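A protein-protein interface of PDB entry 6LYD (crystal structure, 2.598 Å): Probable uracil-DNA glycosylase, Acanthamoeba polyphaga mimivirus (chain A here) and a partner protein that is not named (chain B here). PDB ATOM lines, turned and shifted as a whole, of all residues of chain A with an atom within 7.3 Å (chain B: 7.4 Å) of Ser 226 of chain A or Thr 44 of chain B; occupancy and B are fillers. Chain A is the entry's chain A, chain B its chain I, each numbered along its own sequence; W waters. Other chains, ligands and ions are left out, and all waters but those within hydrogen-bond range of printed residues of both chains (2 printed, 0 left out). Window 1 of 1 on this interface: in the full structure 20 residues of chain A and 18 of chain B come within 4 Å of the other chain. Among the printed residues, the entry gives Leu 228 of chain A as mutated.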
ATOM      1  N   PRO A 100      -0.301  26.925  33.495  1.00  0.00           N
ATOM      2  CA  PRO A 100      -0.070  28.333  33.152  1.00  0.00           C
ATOM      3  C   PRO A 100      -1.247  29.042  32.466  1.00  0.00           C
ATOM      4  O   PRO A 100      -1.317  30.270  32.463  1.00  0.00           O
ATOM      5  CB  PRO A 100       1.105  28.243  32.189  1.00  0.00           C
ATOM      6  CG  PRO A 100       0.824  26.961  31.440  1.00  0.00           C
ATOM      7  CD  PRO A 100       0.266  26.017  32.481  1.00  0.00           C
ATOM      8  N   PHE A 115      -2.126  18.921  39.091  1.00  0.00           N
ATOM      9  CA  PHE A 115      -2.831  18.180  38.041  1.00  0.00           C
ATOM     10  C   PHE A 115      -4.353  18.394  37.981  1.00  0.00           C
ATOM     11  O   PHE A 115      -4.992  17.915  37.056  1.00  0.00           O
ATOM     12  CB  PHE A 115      -2.528  16.674  38.166  1.00  0.00           C
ATOM     13  CG  PHE A 115      -1.070  16.332  37.992  1.00  0.00           C
ATOM     14  CD1 PHE A 115      -0.266  16.082  39.093  1.00  0.00           C
ATOM     15  CD2 PHE A 115      -0.500  16.289  36.726  1.00  0.00           C
ATOM     16  CE1 PHE A 115       1.069  15.783  38.937  1.00  0.00           C
ATOM     17  CE2 PHE A 115       0.837  15.994  36.562  1.00  0.00           C
ATOM     18  CZ  PHE A 115       1.621  15.739  37.667  1.00  0.00           C
ATOM     19  N   PRO A 124      -6.214  19.269  30.641  1.00  0.00           N
ATOM     20  CA  PRO A 124      -4.879  19.179  30.044  1.00  0.00           C
ATOM     21  C   PRO A 124      -4.422  17.722  29.929  1.00  0.00           C
ATOM     22  O   PRO A 124      -4.777  16.888  30.771  1.00  0.00           O
ATOM     23  CB  PRO A 124      -4.007  19.980  31.022  1.00  0.00           C
ATOM     24  CG  PRO A 124      -4.993  20.825  31.837  1.00  0.00           C
ATOM     25  CD  PRO A 124      -6.179  19.919  31.960  1.00  0.00           C
ATOM     26  N   LYS A 125      -3.633  17.426  28.903  1.00  0.00           N
ATOM     27  CA  LYS A 125      -3.366  16.045  28.517  1.00  0.00           C
ATOM     28  C   LYS A 125      -2.664  15.228  29.611  1.00  0.00           C
ATOM     29  O   LYS A 125      -2.903  14.012  29.733  1.00  0.00           O
ATOM     30  CB  LYS A 125      -2.554  16.017  27.221  1.00  0.00           C
ATOM     31  CG  LYS A 125      -3.394  16.322  25.989  1.00  0.00           C
ATOM     32  CD  LYS A 125      -4.609  15.410  25.932  1.00  0.00           C
ATOM     33  CE  LYS A 125      -5.658  15.875  24.924  1.00  0.00           C
ATOM     34  NZ  LYS A 125      -6.949  15.150  25.166  1.00  0.00           N
ATOM     35  N   SER A 126      -1.838  15.872  30.433  1.00  0.00           N
ATOM     36  CA  SER A 126      -1.124  15.089  31.418  1.00  0.00           C
ATOM     37  C   SER A 126      -2.151  14.494  32.392  1.00  0.00           C
ATOM     38  O   SER A 126      -2.007  13.336  32.801  1.00  0.00           O
ATOM     39  CB  SER A 126      -0.032  15.913  32.120  1.00  0.00           C
ATOM     40  OG  SER A 126      -0.553  16.626  33.213  1.00  0.00           O
ATOM     41  N   LEU A 127      -3.219  15.240  32.696  1.00  0.00           N
ATOM     42  CA  LEU A 127      -4.311  14.685  33.505  1.00  0.00           C
ATOM     43  C   LEU A 127      -5.115  13.657  32.699  1.00  0.00           C
ATOM     44  O   LEU A 127      -5.572  12.647  33.235  1.00  0.00           O
ATOM     45  CB  LEU A 127      -5.246  15.784  34.030  1.00  0.00           C
ATOM     46  CG  LEU A 127      -6.520  15.314  34.778  1.00  0.00           C
ATOM     47  CD1 LEU A 127      -6.224  14.311  35.864  1.00  0.00           C
ATOM     48  CD2 LEU A 127      -7.299  16.481  35.372  1.00  0.00           C
ATOM     49  N   ASN A 129      -3.859  11.701  30.645  1.00  0.00           N
ATOM     50  CA  ASN A 129      -3.028  10.503  30.672  1.00  0.00           C
ATOM     51  C   ASN A 129      -3.170   9.766  32.012  1.00  0.00           C
ATOM     52  O   ASN A 129      -3.132   8.528  32.039  1.00  0.00           O
ATOM     53  CB  ASN A 129      -1.560  10.859  30.343  1.00  0.00           C
ATOM     54  CG  ASN A 129      -1.382  11.181  28.863  1.00  0.00           C
ATOM     55  OD1 ASN A 129      -2.228  10.801  28.067  1.00  0.00           O
ATOM     56  ND2 ASN A 129      -0.323  11.906  28.498  1.00  0.00           N
ATOM     57  N   SER A 171       5.518  30.005  32.286  1.00  0.00           N
ATOM     58  CA  SER A 171       5.897  28.786  32.998  1.00  0.00           C
ATOM     59  C   SER A 171       7.253  28.886  33.675  1.00  0.00           C
ATOM     60  O   SER A 171       8.118  29.636  33.250  1.00  0.00           O
ATOM     61  CB  SER A 171       5.897  27.588  32.053  1.00  0.00           C
ATOM     62  OG  SER A 171       4.670  27.479  31.353  1.00  0.00           O
ATOM     63  N   SER A 223       8.174   7.888  34.860  1.00  0.00           N
ATOM     64  CA  SER A 223       8.228   9.099  34.052  1.00  0.00           C
ATOM     65  C   SER A 223       7.003   9.974  34.326  1.00  0.00           C
ATOM     66  O   SER A 223       6.041   9.546  34.962  1.00  0.00           O
ATOM     67  CB  SER A 223       8.323   8.767  32.566  1.00  0.00           C
ATOM     68  OG  SER A 223       7.082   8.356  32.043  1.00  0.00           O
ATOM     69  N   HIS A 224       7.059  11.211  33.857  1.00  0.00           N
ATOM     70  CA  HIS A 224       6.004  12.184  34.083  1.00  0.00           C
ATOM     71  C   HIS A 224       4.867  11.985  33.054  1.00  0.00           C
ATOM     72  O   HIS A 224       5.111  11.616  31.907  1.00  0.00           O
ATOM     73  CB  HIS A 224       6.616  13.589  34.014  1.00  0.00           C
ATOM     74  CG  HIS A 224       5.651  14.690  34.305  1.00  0.00           C
ATOM     75  ND1 HIS A 224       4.652  15.057  33.428  1.00  0.00           N
ATOM     76  CD2 HIS A 224       5.527  15.504  35.377  1.00  0.00           C
ATOM     77  CE1 HIS A 224       3.949  16.045  33.949  1.00  0.00           C
ATOM     78  NE2 HIS A 224       4.457  16.332  35.133  1.00  0.00           N
ATOM     79  N   PRO A 225       3.610  12.220  33.467  1.00  0.00           N
ATOM     80  CA  PRO A 225       2.472  11.981  32.565  1.00  0.00           C
ATOM     81  C   PRO A 225       2.310  12.968  31.389  1.00  0.00           C
ATOM     82  O   PRO A 225       1.409  12.764  30.575  1.00  0.00           O
ATOM     83  CB  PRO A 225       1.273  12.087  33.495  1.00  0.00           C
ATOM     84  CG  PRO A 225       1.745  13.002  34.582  1.00  0.00           C
ATOM     85  CD  PRO A 225       3.162  12.603  34.816  1.00  0.00           C
ATOM     86  N   SER A 226       3.146  13.998  31.297  1.00  0.00           N
ATOM     87  CA  SER A 226       3.128  14.887  30.136  1.00  0.00           C
ATOM     88  C   SER A 226       3.334  14.127  28.816  1.00  0.00           C
ATOM     89  O   SER A 226       4.085  13.155  28.756  1.00  0.00           O
ATOM     90  CB  SER A 226       4.193  15.972  30.275  1.00  0.00           C
ATOM     91  OG  SER A 226       3.793  17.124  29.551  1.00  0.00           O
ATOM     92  N   PRO A 227       2.636  14.546  27.767  1.00  0.00           N
ATOM     93  CA  PRO A 227       2.662  13.885  26.450  1.00  0.00           C
ATOM     94  C   PRO A 227       4.049  13.427  25.959  1.00  0.00           C
ATOM     95  O   PRO A 227       4.200  12.296  25.485  1.00  0.00           O
ATOM     96  CB  PRO A 227       2.093  14.965  25.525  1.00  0.00           C
ATOM     97  CG  PRO A 227       1.105  15.699  26.407  1.00  0.00           C
ATOM     98  CD  PRO A 227       1.565  15.555  27.857  1.00  0.00           C
ATOM     99  N   LEU A 228       5.044  14.297  26.083  1.00  0.00           N
ATOM    100  CA  LEU A 228       6.409  13.965  25.697  1.00  0.00           C
ATOM    101  C   LEU A 228       7.073  12.877  26.569  1.00  0.00           C
ATOM    102  O   LEU A 228       8.022  12.218  26.115  1.00  0.00           O
ATOM    103  CB  LEU A 228       7.263  15.223  25.732  1.00  0.00           C
ATOM    104  CG  LEU A 228       8.551  15.221  24.918  1.00  0.00           C
ATOM    105  CD1 LEU A 228       8.257  15.036  23.437  1.00  0.00           C
ATOM    106  CD2 LEU A 228       9.313  16.510  25.147  1.00  0.00           C
ATOM    107  N   SER A 229       6.593  12.691  27.803  1.00  0.00           N
ATOM    108  CA  SER A 229       7.244  11.763  28.733  1.00  0.00           C
ATOM    109  C   SER A 229       6.492  10.449  28.927  1.00  0.00           C
ATOM    110  O   SER A 229       7.130   9.474  29.306  1.00  0.00           O
ATOM    111  CB  SER A 229       7.415  12.361  30.140  1.00  0.00           C
ATOM    112  OG  SER A 229       7.772  13.717  30.137  1.00  0.00           O
ATOM    113  N   VAL A 230       5.160  10.439  28.724  1.00  0.00           N
ATOM    114  CA  VAL A 230       4.303   9.344  29.219  1.00  0.00           C
ATOM    115  C   VAL A 230       4.824   7.991  28.880  1.00  0.00           C
ATOM    116  O   VAL A 230       4.685   7.061  29.668  1.00  0.00           O
ATOM    117  CB  VAL A 230       2.847   9.372  28.684  1.00  0.00           C
ATOM    118  CG1 VAL A 230       1.860   9.581  29.834  1.00  0.00           C
ATOM    119  CG2 VAL A 230       2.664  10.317  27.501  1.00  0.00           C
ATOM    120  N   SER A 231       5.362   7.883  27.671  1.00  0.00           N
ATOM    121  CA  SER A 231       5.721   6.589  27.104  1.00  0.00           C
ATOM    122  C   SER A 231       7.193   6.292  27.254  1.00  0.00           C
ATOM    123  O   SER A 231       7.636   5.215  26.889  1.00  0.00           O
ATOM    124  CB  SER A 231       5.353   6.537  25.630  1.00  0.00           C
ATOM    125  OG  SER A 231       3.981   6.793  25.491  1.00  0.00           O
ATOM    126  N   ASN A 232       7.945   7.245  27.784  1.00  0.00           N
ATOM    127  CA  ASN A 232       9.380   7.077  27.895  1.00  0.00           C
ATOM    128  C   ASN A 232       9.766   6.700  29.298  1.00  0.00           C
ATOM    129  O   ASN A 232       9.034   6.966  30.244  1.00  0.00           O
ATOM    130  CB  ASN A 232      10.118   8.348  27.487  1.00  0.00           C
ATOM    131  CG  ASN A 232       9.768   8.779  26.101  1.00  0.00           C
ATOM    132  OD1 ASN A 232       9.582   9.965  25.845  1.00  0.00           O
ATOM    133  ND2 ASN A 232       9.653   7.811  25.188  1.00  0.00           N
ATOM    134  N   PHE A 251       5.383   6.226  32.684  1.00  0.00           N
ATOM    135  CA  PHE A 251       4.154   6.455  33.408  1.00  0.00           C
ATOM    136  C   PHE A 251       3.018   5.495  33.013  1.00  0.00           C
ATOM    137  O   PHE A 251       2.313   4.984  33.879  1.00  0.00           O
ATOM    138  CB  PHE A 251       3.710   7.910  33.222  1.00  0.00           C
ATOM    139  CG  PHE A 251       2.422   8.223  33.912  1.00  0.00           C
ATOM    140  CD1 PHE A 251       1.194   7.985  33.278  1.00  0.00           C
ATOM    141  CD2 PHE A 251       2.426   8.704  35.220  1.00  0.00           C
ATOM    142  CE1 PHE A 251      -0.002   8.243  33.933  1.00  0.00           C
ATOM    143  CE2 PHE A 251       1.247   8.970  35.869  1.00  0.00           C
ATOM    144  CZ  PHE A 251       0.022   8.742  35.236  1.00  0.00           C
ATOM    145  N   ILE B   7       4.521  29.215  17.874  1.00  0.00           N
ATOM    146  CA  ILE B   7       3.879  27.990  17.422  1.00  0.00           C
ATOM    147  C   ILE B   7       3.063  28.261  16.175  1.00  0.00           C
ATOM    148  O   ILE B   7       3.101  27.484  15.208  1.00  0.00           O
ATOM    149  CB  ILE B   7       2.990  27.387  18.523  1.00  0.00           C
ATOM    150  CG1 ILE B   7       3.840  26.896  19.691  1.00  0.00           C
ATOM    151  CG2 ILE B   7       2.102  26.275  17.967  1.00  0.00           C
ATOM    152  CD1 ILE B   7       3.023  26.285  20.783  1.00  0.00           C
ATOM    153  N   VAL B  16      -3.598  27.098  22.629  1.00  0.00           N
ATOM    154  CA  VAL B  16      -3.424  27.460  24.034  1.00  0.00           C
ATOM    155  C   VAL B  16      -2.414  26.539  24.719  1.00  0.00           C
ATOM    156  O   VAL B  16      -2.624  25.323  24.763  1.00  0.00           O
ATOM    157  CB  VAL B  16      -4.769  27.409  24.765  1.00  0.00           C
ATOM    158  CG1 VAL B  16      -4.593  27.689  26.245  1.00  0.00           C
ATOM    159  CG2 VAL B  16      -5.714  28.396  24.149  1.00  0.00           C
ATOM    160  N   ILE B  17      -1.324  27.108  25.242  1.00  0.00           N
ATOM    161  CA  ILE B  17      -0.383  26.349  26.068  1.00  0.00           C
ATOM    162  C   ILE B  17      -1.086  25.922  27.341  1.00  0.00           C
ATOM    163  O   ILE B  17      -1.485  26.767  28.134  1.00  0.00           O
ATOM    164  CB  ILE B  17       0.878  27.164  26.404  1.00  0.00           C
ATOM    165  CG1 ILE B  17       1.606  27.580  25.127  1.00  0.00           C
ATOM    166  CG2 ILE B  17       1.788  26.395  27.374  1.00  0.00           C
ATOM    167  CD1 ILE B  17       1.668  26.500  24.116  1.00  0.00           C
ATOM    168  N   GLN B  18      -1.237  24.620  27.548  1.00  0.00           N
ATOM    169  CA  GLN B  18      -1.957  24.142  28.715  1.00  0.00           C
ATOM    170  C   GLN B  18      -1.032  23.718  29.853  1.00  0.00           C
ATOM    171  O   GLN B  18      -1.450  23.696  31.003  1.00  0.00           O
ATOM    172  CB  GLN B  18      -2.877  22.975  28.350  1.00  0.00           C
ATOM    173  CG  GLN B  18      -3.788  23.228  27.156  1.00  0.00           C
ATOM    174  CD  GLN B  18      -4.975  22.269  27.115  1.00  0.00           C
ATOM    175  OE1 GLN B  18      -6.078  22.584  27.583  1.00  0.00           O
ATOM    176  NE2 GLN B  18      -4.754  21.095  26.552  1.00  0.00           N
ATOM    177  N   GLU B  19       0.216  23.380  29.561  1.00  0.00           N
ATOM    178  CA  GLU B  19       1.096  22.882  30.620  1.00  0.00           C
ATOM    179  C   GLU B  19       2.568  22.935  30.219  1.00  0.00           C
ATOM    180  O   GLU B  19       2.910  23.122  29.052  1.00  0.00           O
ATOM    181  CB  GLU B  19       0.709  21.445  31.002  1.00  0.00           C
ATOM    182  CG  GLU B  19       0.908  20.421  29.871  1.00  0.00           C
ATOM    183  CD  GLU B  19       0.615  18.979  30.292  1.00  0.00           C
ATOM    184  OE1 GLU B  19      -0.518  18.493  30.045  1.00  0.00           O
ATOM    185  OE2 GLU B  19       1.519  18.331  30.878  1.00  0.00           O
ATOM    186  N   SER B  20       3.442  22.766  31.193  1.00  0.00           N
ATOM    187  CA  SER B  20       4.874  22.760  30.933  1.00  0.00           C
ATOM    188  C   SER B  20       5.600  21.723  31.805  1.00  0.00           C
ATOM    189  O   SER B  20       5.056  21.285  32.821  1.00  0.00           O
ATOM    190  CB  SER B  20       5.458  24.143  31.191  1.00  0.00           C
ATOM    191  OG  SER B  20       5.732  24.295  32.584  1.00  0.00           O
ATOM    192  N   ILE B  21       6.810  21.326  31.407  1.00  0.00           N
ATOM    193  CA  ILE B  21       7.714  20.634  32.334  1.00  0.00           C
ATOM    194  C   ILE B  21       9.095  21.172  32.076  1.00  0.00           C
ATOM    195  O   ILE B  21       9.380  21.649  30.983  1.00  0.00           O
ATOM    196  CB  ILE B  21       7.708  19.077  32.197  1.00  0.00           C
ATOM    197  CG1 ILE B  21       7.897  18.656  30.731  1.00  0.00           C
ATOM    198  CG2 ILE B  21       6.462  18.449  32.846  1.00  0.00           C
ATOM    199  CD1 ILE B  21       8.277  17.183  30.537  1.00  0.00           C
ATOM    200  N   LEU B  41      12.376  24.108  28.911  1.00  0.00           N
ATOM    201  CA  LEU B  41      10.953  24.063  29.198  1.00  0.00           C
ATOM    202  C   LEU B  41      10.190  23.466  28.021  1.00  0.00           C
ATOM    203  O   LEU B  41      10.334  23.909  26.887  1.00  0.00           O
ATOM    204  CB  LEU B  41      10.421  25.469  29.502  1.00  0.00           C
ATOM    205  CG  LEU B  41      10.792  26.079  30.853  1.00  0.00           C
ATOM    206  CD1 LEU B  41      10.472  27.546  30.813  1.00  0.00           C
ATOM    207  CD2 LEU B  41      10.032  25.405  31.985  1.00  0.00           C
ATOM    208  N   VAL B  42       9.399  22.443  28.297  1.00  0.00           N
ATOM    209  CA  VAL B  42       8.496  21.885  27.306  1.00  0.00           C
ATOM    210  C   VAL B  42       7.135  22.547  27.447  1.00  0.00           C
ATOM    211  O   VAL B  42       6.439  22.307  28.431  1.00  0.00           O
ATOM    212  CB  VAL B  42       8.352  20.368  27.460  1.00  0.00           C
ATOM    213  CG1 VAL B  42       7.434  19.823  26.371  1.00  0.00           C
ATOM    214  CG2 VAL B  42       9.717  19.679  27.459  1.00  0.00           C
ATOM    215  N   HIS B  43       6.761  23.377  26.476  1.00  0.00           N
ATOM    216  CA  HIS B  43       5.468  24.056  26.497  1.00  0.00           C
ATOM    217  C   HIS B  43       4.461  23.230  25.712  1.00  0.00           C
ATOM    218  O   HIS B  43       4.577  23.087  24.492  1.00  0.00           O
ATOM    219  CB  HIS B  43       5.575  25.472  25.915  1.00  0.00           C
ATOM    220  CG  HIS B  43       6.610  26.327  26.585  1.00  0.00           C
ATOM    221  ND1 HIS B  43       6.364  27.022  27.750  1.00  0.00           N
ATOM    222  CD2 HIS B  43       7.889  26.606  26.244  1.00  0.00           C
ATOM    223  CE1 HIS B  43       7.448  27.696  28.097  1.00  0.00           C
ATOM    224  NE2 HIS B  43       8.390  27.455  27.203  1.00  0.00           N
ATOM    225  N   THR B  44       3.475  22.674  26.402  1.00  0.00           N
ATOM    226  CA  THR B  44       2.609  21.722  25.732  1.00  0.00           C
ATOM    227  C   THR B  44       1.235  22.283  25.443  1.00  0.00           C
ATOM    228  O   THR B  44       0.539  22.793  26.318  1.00  0.00           O
ATOM    229  CB  THR B  44       2.478  20.420  26.540  1.00  0.00           C
ATOM    230  OG1 THR B  44       3.770  19.810  26.630  1.00  0.00           O
ATOM    231  CG2 THR B  44       1.519  19.455  25.869  1.00  0.00           C
ATOM    232  N   ALA B  45       0.872  22.187  24.176  1.00  0.00           N
ATOM    233  CA  ALA B  45      -0.448  22.557  23.718  1.00  0.00           C
ATOM    234  C   ALA B  45      -1.115  21.345  23.081  1.00  0.00           C
ATOM    235  O   ALA B  45      -0.431  20.425  22.600  1.00  0.00           O
ATOM    236  CB  ALA B  45      -0.359  23.703  22.730  1.00  0.00           C
ATOM    237  N   TYR B  46      -2.444  21.344  23.079  1.00  0.00           N
ATOM    238  CA  TYR B  46      -3.191  20.342  22.331  1.00  0.00           C
ATOM    239  C   TYR B  46      -3.937  20.960  21.158  1.00  0.00           C
ATOM    240  O   TYR B  46      -4.518  22.030  21.290  1.00  0.00           O
ATOM    241  CB  TYR B  46      -4.185  19.622  23.222  1.00  0.00           C
ATOM    242  CG  TYR B  46      -4.875  18.485  22.520  1.00  0.00           C
ATOM    243  CD1 TYR B  46      -4.142  17.532  21.828  1.00  0.00           C
ATOM    244  CD2 TYR B  46      -6.268  18.359  22.540  1.00  0.00           C
ATOM    245  CE1 TYR B  46      -4.778  16.464  21.189  1.00  0.00           C
ATOM    246  CE2 TYR B  46      -6.903  17.303  21.906  1.00  0.00           C
ATOM    247  CZ  TYR B  46      -6.155  16.361  21.234  1.00  0.00           C
ATOM    248  OH  TYR B  46      -6.778  15.320  20.600  1.00  0.00           O
ATOM    249  N   ASN B  53      -0.283  16.464  19.827  1.00  0.00           N
ATOM    250  CA  ASN B  53       0.268  17.284  20.894  1.00  0.00           C
ATOM    251  C   ASN B  53       1.341  18.133  20.270  1.00  0.00           C
ATOM    252  O   ASN B  53       2.207  17.632  19.574  1.00  0.00           O
ATOM    253  CB  ASN B  53       0.817  16.447  22.047  1.00  0.00           C
ATOM    254  CG  ASN B  53      -0.177  15.412  22.543  1.00  0.00           C
ATOM    255  OD1 ASN B  53      -1.264  15.759  22.998  1.00  0.00           O
ATOM    256  ND2 ASN B  53       0.194  14.130  22.462  1.00  0.00           N
ATOM    257  N   VAL B  54       1.252  19.436  20.480  1.00  0.00           N
ATOM    258  CA  VAL B  54       2.235  20.326  19.929  1.00  0.00           C
ATOM    259  C   VAL B  54       3.073  20.879  21.061  1.00  0.00           C
ATOM    260  O   VAL B  54       2.573  21.594  21.927  1.00  0.00           O
ATOM    261  CB  VAL B  54       1.572  21.431  19.124  1.00  0.00           C
ATOM    262  CG1 VAL B  54       2.576  22.538  18.791  1.00  0.00           C
ATOM    263  CG2 VAL B  54       0.968  20.851  17.875  1.00  0.00           C
ATOM    264  N   MET B  55       4.354  20.551  21.063  1.00  0.00           N
ATOM    265  CA  MET B  55       5.204  21.010  22.146  1.00  0.00           C
ATOM    266  C   MET B  55       6.375  21.864  21.693  1.00  0.00           C
ATOM    267  O   MET B  55       7.224  21.439  20.908  1.00  0.00           O
ATOM    268  CB  MET B  55       5.673  19.814  22.934  1.00  0.00           C
ATOM    269  CG  MET B  55       4.480  19.130  23.582  1.00  0.00           C
ATOM    270  SD  MET B  55       4.549  17.356  23.546  1.00  0.00           S
ATOM    271  CE  MET B  55       4.819  16.978  21.823  1.00  0.00           C
ATOM    272  N   LEU B  56       6.389  23.093  22.192  1.00  0.00           N
ATOM    273  CA  LEU B  56       7.456  24.039  21.923  1.00  0.00           C
ATOM    274  C   LEU B  56       8.500  23.958  23.026  1.00  0.00           C
ATOM    275  O   LEU B  56       8.177  24.043  24.207  1.00  0.00           O
ATOM    276  CB  LEU B  56       6.900  25.457  21.813  1.00  0.00           C
ATOM    277  CG  LEU B  56       7.911  26.591  21.728  1.00  0.00           C
ATOM    278  CD1 LEU B  56       8.583  26.554  20.376  1.00  0.00           C
ATOM    279  CD2 LEU B  56       7.227  27.918  21.947  1.00  0.00           C
ATOM    280  N   LEU B  57       9.753  23.791  22.623  1.00  0.00           N
ATOM    281  CA  LEU B  57      10.853  23.562  23.547  1.00  0.00           C
ATOM    282  C   LEU B  57      11.737  24.812  23.603  1.00  0.00           C
ATOM    283  O   LEU B  57      12.314  25.230  22.587  1.00  0.00           O
ATOM    284  CB  LEU B  57      11.663  22.324  23.117  1.00  0.00           C
ATOM    285  CG  LEU B  57      11.130  20.949  23.549  1.00  0.00           C
ATOM    286  CD1 LEU B  57       9.738  20.618  22.977  1.00  0.00           C
ATOM    287  CD2 LEU B  57      12.150  19.843  23.250  1.00  0.00           C
ATOM    288  N   GLN B  72       3.478  15.571  17.875  1.00  0.00           N
ATOM    289  CA  GLN B  72       3.278  14.180  18.225  1.00  0.00           C
ATOM    290  C   GLN B  72       1.834  13.741  17.934  1.00  0.00           C
ATOM    291  O   GLN B  72       0.871  14.368  18.380  1.00  0.00           O
ATOM    292  CB  GLN B  72       3.638  13.969  19.686  1.00  0.00           C
ATOM    293  CG  GLN B  72       3.380  12.584  20.219  1.00  0.00           C
ATOM    294  CD  GLN B  72       3.612  12.517  21.717  1.00  0.00           C
ATOM    295  OE1 GLN B  72       2.661  12.567  22.516  1.00  0.00           O
ATOM    296  NE2 GLN B  72       4.884  12.432  22.115  1.00  0.00           N
HETATM  297  O   HOH W   1       4.942  17.272  27.222  1.00  0.00           O
HETATM  298  O   HOH W   2       7.692  11.530  23.255  1.00  0.00           O
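The backbone carbonyl oxygen (O) of Ser 229 of chain A is in hydrogen-bond range of the side-chain hydroxyl (OG) of Ser 223 of chain A (3.0 Å).
A ring nitrogen (ND1) of His 224 of chain A lies within hydrogen-bond range of the backbone NH (N) of Ser 226 of chain A.
O of Leu 228 of chain A lies close to OD1 of Asn 232 of chain A, 2.8 Å away.
The backbone NH (N) of Gln 18 of chain B sits at hydrogen-bond distance from the backbone carbonyl oxygen (O) of Thr 44 of chain B (2.8 Å).
The backbone carbonyl oxygen (O) of Glu 19 of chain B sits at hydrogen-bond distance from the backbone NH (N) of Thr 44 of chain B (2.7 Å).
The backbone carbonyl oxygen (O) of Ile 21 of chain B sits at hydrogen-bond distance from the backbone NH (N) of Val 42 of chain B, at 2.8 Å.
Among the printed residues, pairs that only touch across the chains: Pro 100 of chain A with Gln 18 of chain B, Ser 171 of chain A with Ser 20 of chain B, Lys 125 of chain A with Tyr 46 of chain B, Ser 229 of chain A with Ile 21 of chain B, His 224 of chain A with Ile 21 of chain B, Pro 227 of chain A with Asn 53 of chain B, Lys 125 of chain A with Asn 53 of chain B, Pro 100 of chain A with Glu 19 of chain B, Pro 227 of chain A with Thr 44 of chain B, Pro 124 of chain A with Glu 19 of chain B, Leu 228 of chain A with Val 42 of chain B, Pro 227 of chain A with Met 55 of chain B, Ser 226 of chain A with Thr 44 of chain B, Ser 171 of chain A with Leu 41 of chain B and Pro 124 of chain A with Gln 18 of chain B.
Water W1 lies within hydrogen-bond range of OG of Ser 226 of chain A, OG1 of Thr 44 of chain B, N of Leu 228 of chain A and SD of Met 55 of chain B.
Water W2 lies within hydrogen-bond range of O of Leu 228 of chain A and NE2 of Gln 72 of chain B.
Of the 19 printed residues of chain A, 10 touch a printed residue of chain B.
Hydrophobic or aromatic side chains of chain B within 4 Å of the printed part of chain A: Ile 21, Leu 41, Val 42, Tyr 46 and Met 55.
Among the printed residues, 19 pairs touch across the chains.
N of Lys 125 of chain A lies within hydrogen-bond range of OE1 of Glu 19 of chain B (3.5 Å).
The backbone NH (N) of Ser 126 of chain A lies within hydrogen-bond range of the side-chain carboxylate (OE1) of Glu 19 of chain B, at 3.0 Å.
The side-chain hydroxyl (OG) of Ser 226 of chain A sits at hydrogen-bond distance from the side-chain carboxylate (OE2) of Glu 19 of chain B.
The side-chain amide oxygen (OE1) of Gln 72 of chain B lies close to the backbone carbonyl oxygen (O) of Pro 227 of chain A, 3.4 Å away.
Of chain B, only Glu 19 (2.9 Å) and Thr 44 (3.97 Å) come within 4 Å of Ser 226 of chain A.
Of the printed residues of chain A, Thr 44 of chain B touches Ser 226 (3.97 Å) and Pro 227 (3.8 Å).
Of the printed residues of chain B, Ser 229 of chain A touches Ile 21.
Of the printed residues of chain A, Asn 53 of chain B touches Lys 125 (3.7 Å) and Pro 227 (3.7 Å).
Of the printed residues of chain A, Glu 19 of chain B touches Pro 100 (3.7 Å), Pro 124 (3.9 Å), Lys 125 (3.5 Å), Ser 126 (3.0 Å) and Ser 226 (2.9 Å).
Printed residues of chain A within 4 Å of Ser 20 of chain B: Ser 171 (3.3 Å).
Printed residues of chain B within 4 Å of Pro 100 of chain A: Gln 18 (3.2 Å) and Glu 19 (3.7 Å).
Ser 231 of chain A touches none of the printed residues of chain B.
Val 54 of chain B touches none of the printed residues of chain A.
The nearest residue of chain A that does not touch Thr 44 of chain B is Lys 125 of chain A (5.5 Å).
The nearest printed residue of chain A that does not touch Tyr 46 of chain B is Pro 124 of chain A (6.9 Å).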
